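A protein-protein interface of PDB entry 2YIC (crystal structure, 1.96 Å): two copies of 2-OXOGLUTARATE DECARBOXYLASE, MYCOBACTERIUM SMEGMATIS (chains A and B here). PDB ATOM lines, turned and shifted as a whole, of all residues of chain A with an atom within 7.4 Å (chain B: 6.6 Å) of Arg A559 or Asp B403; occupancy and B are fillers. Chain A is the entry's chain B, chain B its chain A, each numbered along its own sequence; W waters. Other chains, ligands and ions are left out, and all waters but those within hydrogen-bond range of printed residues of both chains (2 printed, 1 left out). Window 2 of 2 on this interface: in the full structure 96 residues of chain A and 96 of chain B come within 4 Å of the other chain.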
ATOM      1  N   PHE A 495       3.098  23.062   2.484  1.00  0.00           N
ATOM      2  CA  PHE A 495       2.181  21.938   2.700  1.00  0.00           C
ATOM      3  C   PHE A 495       2.453  21.327   4.058  1.00  0.00           C
ATOM      4  O   PHE A 495       3.614  21.109   4.402  1.00  0.00           O
ATOM      5  CB  PHE A 495       2.303  20.885   1.587  1.00  0.00           C
ATOM      6  CG  PHE A 495       1.193  19.867   1.568  1.00  0.00           C
ATOM      7  CD1 PHE A 495       1.266  18.715   2.352  1.00  0.00           C
ATOM      8  CD2 PHE A 495       0.087  20.039   0.745  1.00  0.00           C
ATOM      9  CE1 PHE A 495       0.223  17.778   2.348  1.00  0.00           C
ATOM     10  CE2 PHE A 495      -0.946  19.090   0.725  1.00  0.00           C
ATOM     11  CZ  PHE A 495      -0.866  17.965   1.523  1.00  0.00           C
ATOM     12  N   THR A 496       1.392  21.076   4.842  1.00  0.00           N
ATOM     13  CA  THR A 496       1.533  20.478   6.174  1.00  0.00           C
ATOM     14  C   THR A 496       1.030  19.055   6.134  1.00  0.00           C
ATOM     15  O   THR A 496      -0.171  18.826   6.000  1.00  0.00           O
ATOM     16  CB  THR A 496       0.811  21.312   7.252  1.00  0.00           C
ATOM     17  OG1 THR A 496       1.174  22.691   7.115  1.00  0.00           O
ATOM     18  CG2 THR A 496       1.139  20.841   8.671  1.00  0.00           C
ATOM     19  N   VAL A 497       1.953  18.089   6.235  1.00  0.00           N
ATOM     20  CA  VAL A 497       1.616  16.660   6.228  1.00  0.00           C
ATOM     21  C   VAL A 497       1.095  16.273   7.593  1.00  0.00           C
ATOM     22  O   VAL A 497       1.635  16.741   8.602  1.00  0.00           O
ATOM     23  CB  VAL A 497       2.830  15.779   5.830  1.00  0.00           C
ATOM     24  CG1 VAL A 497       2.424  14.312   5.635  1.00  0.00           C
ATOM     25  CG2 VAL A 497       3.474  16.301   4.566  1.00  0.00           C
ATOM     26  N   HIS A 498       0.060  15.413   7.638  1.00  0.00           N
ATOM     27  CA  HIS A 498      -0.457  14.868   8.894  1.00  0.00           C
ATOM     28  C   HIS A 498       0.676  14.109   9.619  1.00  0.00           C
ATOM     29  O   HIS A 498       1.383  13.325   8.972  1.00  0.00           O
ATOM     30  CB  HIS A 498      -1.642  13.915   8.623  1.00  0.00           C
ATOM     31  CG  HIS A 498      -2.353  13.502   9.869  1.00  0.00           C
ATOM     32  ND1 HIS A 498      -1.845  12.519  10.696  1.00  0.00           N
ATOM     33  CD2 HIS A 498      -3.531  13.937  10.372  1.00  0.00           C
ATOM     34  CE1 HIS A 498      -2.706  12.415  11.692  1.00  0.00           C
ATOM     35  NE2 HIS A 498      -3.755  13.220  11.518  1.00  0.00           N
ATOM     36  N   PRO A 499       0.856  14.306  10.949  1.00  0.00           N
ATOM     37  CA  PRO A 499       1.949  13.618  11.664  1.00  0.00           C
ATOM     38  C   PRO A 499       2.017  12.097  11.474  1.00  0.00           C
ATOM     39  O   PRO A 499       3.124  11.563  11.513  1.00  0.00           O
ATOM     40  CB  PRO A 499       1.670  13.951  13.131  1.00  0.00           C
ATOM     41  CG  PRO A 499       0.952  15.232  13.084  1.00  0.00           C
ATOM     42  CD  PRO A 499       0.112  15.204  11.854  1.00  0.00           C
ATOM     43  N   ILE A 556      -2.671  12.757  -0.279  1.00  0.00           N
ATOM     44  CA  ILE A 556      -2.439  13.138   1.117  1.00  0.00           C
ATOM     45  C   ILE A 556      -3.121  14.493   1.329  1.00  0.00           C
ATOM     46  O   ILE A 556      -3.271  15.267   0.382  1.00  0.00           O
ATOM     47  CB  ILE A 556      -0.975  13.062   1.582  1.00  0.00           C
ATOM     48  CG1 ILE A 556      -0.092  14.114   0.904  1.00  0.00           C
ATOM     49  CG2 ILE A 556      -0.427  11.619   1.404  1.00  0.00           C
ATOM     50  CD1 ILE A 556       1.186  14.408   1.652  1.00  0.00           C
ATOM     51  N   VAL A 557      -3.630  14.722   2.548  1.00  0.00           N
ATOM     52  CA  VAL A 557      -4.446  15.885   2.858  1.00  0.00           C
ATOM     53  C   VAL A 557      -3.706  16.838   3.810  1.00  0.00           C
ATOM     54  O   VAL A 557      -3.258  16.428   4.892  1.00  0.00           O
ATOM     55  CB  VAL A 557      -5.826  15.418   3.429  1.00  0.00           C
ATOM     56  CG1 VAL A 557      -6.725  16.599   3.776  1.00  0.00           C
ATOM     57  CG2 VAL A 557      -6.540  14.468   2.450  1.00  0.00           C
ATOM     58  N   ASP A 558      -3.606  18.123   3.399  1.00  0.00           N
ATOM     59  CA  ASP A 558      -2.967  19.154   4.226  1.00  0.00           C
ATOM     60  C   ASP A 558      -3.714  19.233   5.565  1.00  0.00           C
ATOM     61  O   ASP A 558      -4.945  19.369   5.583  1.00  0.00           O
ATOM     62  CB  ASP A 558      -2.927  20.509   3.500  1.00  0.00           C
ATOM     63  CG  ASP A 558      -2.102  21.582   4.202  1.00  0.00           C
ATOM     64  OD1 ASP A 558      -2.466  21.970   5.319  1.00  0.00           O
ATOM     65  OD2 ASP A 558      -1.086  22.019   3.631  1.00  0.00           O
ATOM     66  N   ARG A 559      -2.971  19.014   6.654  1.00  0.00           N
ATOM     67  CA  ARG A 559      -3.456  19.001   8.030  1.00  0.00           C
ATOM     68  C   ARG A 559      -4.102  20.352   8.424  1.00  0.00           C
ATOM     69  O   ARG A 559      -5.021  20.355   9.242  1.00  0.00           O
ATOM     70  CB  ARG A 559      -2.270  18.669   8.998  1.00  0.00           C
ATOM     71  CG  ARG A 559      -2.603  18.591  10.501  1.00  0.00           C
ATOM     72  CD  ARG A 559      -3.584  17.448  10.761  1.00  0.00           C
ATOM     73  NE  ARG A 559      -4.176  17.427  12.104  1.00  0.00           N
ATOM     74  CZ  ARG A 559      -5.218  18.173  12.476  1.00  0.00           C
ATOM     75  NH1 ARG A 559      -5.729  19.072  11.649  1.00  0.00           N
ATOM     76  NH2 ARG A 559      -5.721  18.060  13.695  1.00  0.00           N
ATOM     77  N   LYS A 560      -3.660  21.470   7.803  1.00  0.00           N
ATOM     78  CA  LYS A 560      -4.144  22.821   8.103  1.00  0.00           C
ATOM     79  C   LYS A 560      -5.177  23.362   7.108  1.00  0.00           C
ATOM     80  O   LYS A 560      -6.116  24.024   7.548  1.00  0.00           O
ATOM     81  CB  LYS A 560      -2.966  23.798   8.165  1.00  0.00           C
ATOM     82  CG  LYS A 560      -2.010  23.545   9.313  1.00  0.00           C
ATOM     83  CD  LYS A 560      -1.434  24.852   9.819  1.00  0.00           C
ATOM     84  CE  LYS A 560       0.055  24.901   9.655  1.00  0.00           C
ATOM     85  NZ  LYS A 560       0.590  26.199  10.128  1.00  0.00           N
ATOM     86  N   THR A 561      -5.038  23.093   5.791  1.00  0.00           N
ATOM     87  CA  THR A 561      -5.958  23.654   4.776  1.00  0.00           C
ATOM     88  C   THR A 561      -6.927  22.645   4.149  1.00  0.00           C
ATOM     89  O   THR A 561      -7.908  23.045   3.509  1.00  0.00           O
ATOM     90  CB  THR A 561      -5.153  24.307   3.633  1.00  0.00           C
ATOM     91  OG1 THR A 561      -4.443  23.282   2.934  1.00  0.00           O
ATOM     92  CG2 THR A 561      -4.184  25.407   4.124  1.00  0.00           C
ATOM     93  N   GLY A 562      -6.616  21.357   4.264  1.00  0.00           N
ATOM     94  CA  GLY A 562      -7.428  20.309   3.667  1.00  0.00           C
ATOM     95  C   GLY A 562      -7.165  20.107   2.187  1.00  0.00           C
ATOM     96  O   GLY A 562      -7.837  19.307   1.554  1.00  0.00           O
ATOM     97  N   GLU A 563      -6.190  20.819   1.627  1.00  0.00           N
ATOM     98  CA  GLU A 563      -5.779  20.704   0.221  1.00  0.00           C
ATOM     99  C   GLU A 563      -5.181  19.325  -0.051  1.00  0.00           C
ATOM    100  O   GLU A 563      -4.422  18.802   0.764  1.00  0.00           O
ATOM    101  CB  GLU A 563      -4.726  21.780  -0.126  1.00  0.00           C
ATOM    102  CG  GLU A 563      -5.241  23.199  -0.210  1.00  0.00           C
ATOM    103  CD  GLU A 563      -4.105  24.184  -0.423  1.00  0.00           C
ATOM    104  OE1 GLU A 563      -3.666  24.346  -1.586  1.00  0.00           O
ATOM    105  OE2 GLU A 563      -3.611  24.748   0.581  1.00  0.00           O
ATOM    106  N   SER B 395      -8.585  12.527  11.331  1.00  0.00           N
ATOM    107  CA  SER B 395      -8.041  13.831  10.960  1.00  0.00           C
ATOM    108  C   SER B 395      -7.003  13.688   9.805  1.00  0.00           C
ATOM    109  O   SER B 395      -6.610  14.706   9.223  1.00  0.00           O
ATOM    110  CB  SER B 395      -7.409  14.520  12.168  1.00  0.00           C
ATOM    111  OG  SER B 395      -6.231  13.833  12.578  1.00  0.00           O
ATOM    112  N   MET B 396      -6.603  12.439   9.458  1.00  0.00           N
ATOM    113  CA  MET B 396      -5.674  12.188   8.331  1.00  0.00           C
ATOM    114  C   MET B 396      -6.330  12.599   7.023  1.00  0.00           C
ATOM    115  O   MET B 396      -5.671  13.208   6.178  1.00  0.00           O
ATOM    116  CB  MET B 396      -5.267  10.699   8.243  1.00  0.00           C
ATOM    117  CG  MET B 396      -4.107  10.312   9.148  1.00  0.00           C
ATOM    118  SD  MET B 396      -3.471   8.648   8.764  1.00  0.00           S
ATOM    119  CE  MET B 396      -4.852   7.643   9.309  1.00  0.00           C
ATOM    120  N   GLN B 398      -9.983  13.859   7.055  1.00  0.00           N
ATOM    121  CA  GLN B 398     -10.978  14.917   7.259  1.00  0.00           C
ATOM    122  C   GLN B 398     -10.511  15.832   8.432  1.00  0.00           C
ATOM    123  O   GLN B 398     -11.175  15.864   9.472  1.00  0.00           O
ATOM    124  CB  GLN B 398     -12.383  14.299   7.494  1.00  0.00           C
ATOM    125  CG  GLN B 398     -12.933  13.460   6.308  1.00  0.00           C
ATOM    126  CD  GLN B 398     -13.018  14.179   4.981  1.00  0.00           C
ATOM    127  OE1 GLN B 398     -13.133  15.416   4.911  1.00  0.00           O
ATOM    128  NE2 GLN B 398     -12.985  13.403   3.887  1.00  0.00           N
ATOM    129  N   PRO B 399      -9.355  16.550   8.295  1.00  0.00           N
ATOM    130  CA  PRO B 399      -8.831  17.333   9.432  1.00  0.00           C
ATOM    131  C   PRO B 399      -9.746  18.448   9.928  1.00  0.00           C
ATOM    132  O   PRO B 399      -9.804  18.652  11.135  1.00  0.00           O
ATOM    133  CB  PRO B 399      -7.513  17.916   8.897  1.00  0.00           C
ATOM    134  CG  PRO B 399      -7.631  17.859   7.410  1.00  0.00           C
ATOM    135  CD  PRO B 399      -8.427  16.621   7.136  1.00  0.00           C
ATOM    136  N   TYR B 400     -10.447  19.154   9.021  1.00  0.00           N
ATOM    137  CA  TYR B 400     -11.341  20.244   9.425  1.00  0.00           C
ATOM    138  C   TYR B 400     -12.515  19.704  10.232  1.00  0.00           C
ATOM    139  O   TYR B 400     -12.779  20.209  11.324  1.00  0.00           O
ATOM    140  CB  TYR B 400     -11.834  21.046   8.210  1.00  0.00           C
ATOM    141  CG  TYR B 400     -12.927  22.040   8.533  1.00  0.00           C
ATOM    142  CD1 TYR B 400     -12.713  23.074   9.441  1.00  0.00           C
ATOM    143  CD2 TYR B 400     -14.174  21.960   7.920  1.00  0.00           C
ATOM    144  CE1 TYR B 400     -13.719  23.987   9.746  1.00  0.00           C
ATOM    145  CE2 TYR B 400     -15.181  22.884   8.204  1.00  0.00           C
ATOM    146  CZ  TYR B 400     -14.951  23.890   9.124  1.00  0.00           C
ATOM    147  OH  TYR B 400     -15.944  24.801   9.414  1.00  0.00           O
ATOM    148  N   MET B 401     -13.214  18.678   9.709  1.00  0.00           N
ATOM    149  CA  MET B 401     -14.338  18.063  10.421  1.00  0.00           C
ATOM    150  C   MET B 401     -13.910  17.573  11.831  1.00  0.00           C
ATOM    151  O   MET B 401     -14.608  17.849  12.815  1.00  0.00           O
ATOM    152  CB  MET B 401     -14.925  16.905   9.588  1.00  0.00           C
ATOM    153  CG  MET B 401     -15.787  15.976  10.412  1.00  0.00           C
ATOM    154  SD  MET B 401     -16.592  14.614   9.540  1.00  0.00           S
ATOM    155  CE  MET B 401     -18.036  15.498   8.880  1.00  0.00           C
ATOM    156  N   TYR B 402     -12.754  16.878  11.926  1.00  0.00           N
ATOM    157  CA  TYR B 402     -12.321  16.327  13.211  1.00  0.00           C
ATOM    158  C   TYR B 402     -11.734  17.351  14.162  1.00  0.00           C
ATOM    159  O   TYR B 402     -11.819  17.140  15.375  1.00  0.00           O
ATOM    160  CB  TYR B 402     -11.460  15.076  13.055  1.00  0.00           C
ATOM    161  CG  TYR B 402     -12.419  13.921  12.834  1.00  0.00           C
ATOM    162  CD1 TYR B 402     -12.928  13.649  11.559  1.00  0.00           C
ATOM    163  CD2 TYR B 402     -12.991  13.253  13.917  1.00  0.00           C
ATOM    164  CE1 TYR B 402     -13.940  12.712  11.365  1.00  0.00           C
ATOM    165  CE2 TYR B 402     -13.973  12.278  13.731  1.00  0.00           C
ATOM    166  CZ  TYR B 402     -14.437  12.006  12.456  1.00  0.00           C
ATOM    167  OH  TYR B 402     -15.457  11.106  12.291  1.00  0.00           O
ATOM    168  N   ASP B 403     -11.273  18.501  13.667  1.00  0.00           N
ATOM    169  CA  ASP B 403     -10.863  19.559  14.598  1.00  0.00           C
ATOM    170  C   ASP B 403     -12.142  20.190  15.210  1.00  0.00           C
ATOM    171  O   ASP B 403     -12.134  20.559  16.382  1.00  0.00           O
ATOM    172  CB  ASP B 403      -9.970  20.601  13.922  1.00  0.00           C
ATOM    173  CG  ASP B 403      -8.534  20.131  13.701  1.00  0.00           C
ATOM    174  OD1 ASP B 403      -8.088  19.221  14.430  1.00  0.00           O
ATOM    175  OD2 ASP B 403      -7.848  20.714  12.847  1.00  0.00           O
ATOM    176  N   VAL B 404     -13.259  20.216  14.452  1.00  0.00           N
ATOM    177  CA  VAL B 404     -14.543  20.723  14.953  1.00  0.00           C
ATOM    178  C   VAL B 404     -15.166  19.667  15.912  1.00  0.00           C
ATOM    179  O   VAL B 404     -15.616  20.046  16.987  1.00  0.00           O
ATOM    180  CB  VAL B 404     -15.511  21.140  13.809  1.00  0.00           C
ATOM    181  CG1 VAL B 404     -16.912  21.487  14.345  1.00  0.00           C
ATOM    182  CG2 VAL B 404     -14.930  22.317  13.032  1.00  0.00           C
ATOM    183  N   ILE B 405     -15.131  18.363  15.559  1.00  0.00           N
ATOM    184  CA  ILE B 405     -15.634  17.266  16.408  1.00  0.00           C
ATOM    185  C   ILE B 405     -14.913  17.230  17.743  1.00  0.00           C
ATOM    186  O   ILE B 405     -15.565  16.975  18.752  1.00  0.00           O
ATOM    187  CB  ILE B 405     -15.543  15.894  15.700  1.00  0.00           C
ATOM    188  CG1 ILE B 405     -16.548  15.844  14.530  1.00  0.00           C
ATOM    189  CG2 ILE B 405     -15.688  14.710  16.716  1.00  0.00           C
ATOM    190  CD1 ILE B 405     -16.581  14.588  13.634  1.00  0.00           C
ATOM    191  N   ASP B 406     -13.593  17.508  17.760  1.00  0.00           N
ATOM    192  CA  ASP B 406     -12.795  17.532  18.993  1.00  0.00           C
ATOM    193  C   ASP B 406     -13.266  18.624  19.971  1.00  0.00           C
ATOM    194  O   ASP B 406     -12.947  18.536  21.153  1.00  0.00           O
ATOM    195  CB  ASP B 406     -11.288  17.697  18.680  1.00  0.00           C
ATOM    196  CG  ASP B 406     -10.564  16.444  18.179  1.00  0.00           C
ATOM    197  OD1 ASP B 406     -11.198  15.363  18.122  1.00  0.00           O
ATOM    198  OD2 ASP B 406      -9.371  16.551  17.826  1.00  0.00           O
ATOM    199  N   THR B 407     -14.031  19.640  19.504  1.00  0.00           N
ATOM    200  CA  THR B 407     -14.539  20.707  20.411  1.00  0.00           C
ATOM    201  C   THR B 407     -15.936  20.361  20.944  1.00  0.00           C
ATOM    202  O   THR B 407     -16.454  21.040  21.832  1.00  0.00           O
ATOM    203  CB  THR B 407     -14.564  22.081  19.723  1.00  0.00           C
ATOM    204  OG1 THR B 407     -15.601  22.116  18.734  1.00  0.00           O
ATOM    205  CG2 THR B 407     -13.204  22.476  19.131  1.00  0.00           C
ATOM    206  N   LYS B 408     -16.545  19.317  20.374  1.00  0.00           N
ATOM    207  CA  LYS B 408     -17.883  18.872  20.728  1.00  0.00           C
ATOM    208  C   LYS B 408     -17.931  18.057  21.995  1.00  0.00           C
ATOM    209  O   LYS B 408     -17.143  17.129  22.186  1.00  0.00           O
ATOM    210  CB  LYS B 408     -18.506  18.032  19.586  1.00  0.00           C
ATOM    211  CG  LYS B 408     -18.717  18.782  18.270  1.00  0.00           C
ATOM    212  CD  LYS B 408     -19.843  19.831  18.326  1.00  0.00           C
ATOM    213  CE  LYS B 408     -21.240  19.257  18.350  1.00  0.00           C
ATOM    214  NZ  LYS B 408     -22.264  20.329  18.471  1.00  0.00           N
HETATM  215  O   HOH W   1      -5.962  15.675  15.169  1.00  0.00           O
HETATM  216  O   HOH W   2      -3.479  12.761   4.576  1.00  0.00           O
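CA of Met B396 touches CD2 of His A498 (3.4 Å). CB of Val A557 touches O of Met B396, 3.5 Å away. CG1 of Val A557 touches CD of Pro B399, 3.8 Å away. O of Asp A558 touches CG of Pro B399, 3.6 Å away. NH1 of Arg A559 touches CB of Pro B399, at 3.5 Å.
The side-chain carboxylate of Asp A558 is in hydrogen-bond range of the backbone NH of Thr A561. N of Arg A559 lies within hydrogen-bond range of O of Thr A496 (2.9 Å). N of Asp A558 lies within hydrogen-bond range of O of Glu A563 (2.8 Å). OD1 of Asp A558 sits at hydrogen-bond distance from N of Lys A560 (2.8 Å). N of Thr A496 is in hydrogen-bond range of OD2 of Asp A558, 2.9 Å away.
Water W2 lies within hydrogen-bond range of the backbone carbonyl oxygen of Met B396 and the backbone NH of Val A557. Water W1 bridges NH2 of Arg A559 (2.8 Å) and OG of Ser B395 (3.2 Å).
No position is printed for both chains.
Hydrophobic or aromatic side chains of chain A within 4 Å of the printed part of chain B: His A498 and Val A557. Along chain A the printed residues that touch a printed residue of chain B span positions 498 to 559. Among the printed residues, 7 pairs touch across the chains.
The side-chain carboxylate (OD1) of Asp B403 lies within salt-bridge range of the guanidinium group (NH2) of Arg A559, at 2.7 Å. The side-chain hydroxyl (OG) of Ser B395 sits at hydrogen-bond distance from a ring nitrogen (NE2) of His A498 (2.8 Å).
Of the printed residues of chain B, Val A557 touches Met B396 (3.5 Å) and Pro B399 (3.8 Å). Of the printed residues of chain B, Asp A558 touches Pro B399. Arg A559 touches just these residues of chain B: Pro B399 and Asp B403. Printed residues of chain A within 4 Å of Ser B395: His A498. Of the printed residues of chain A, Pro B399 touches Val A557 (3.8 Å), Asp A558 (3.6 Å) and Arg A559 (3.5 Å). Tyr B400 touches none of the printed residues of chain A. Tyr B402 touches none of the printed residues of chain A. The nearest residue of chain B that does not touch Arg A559 is Ser B395 (4.2 Å). The nearest residue of chain A that does not touch Asp B403 is Lys A560 (6.4 Å).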
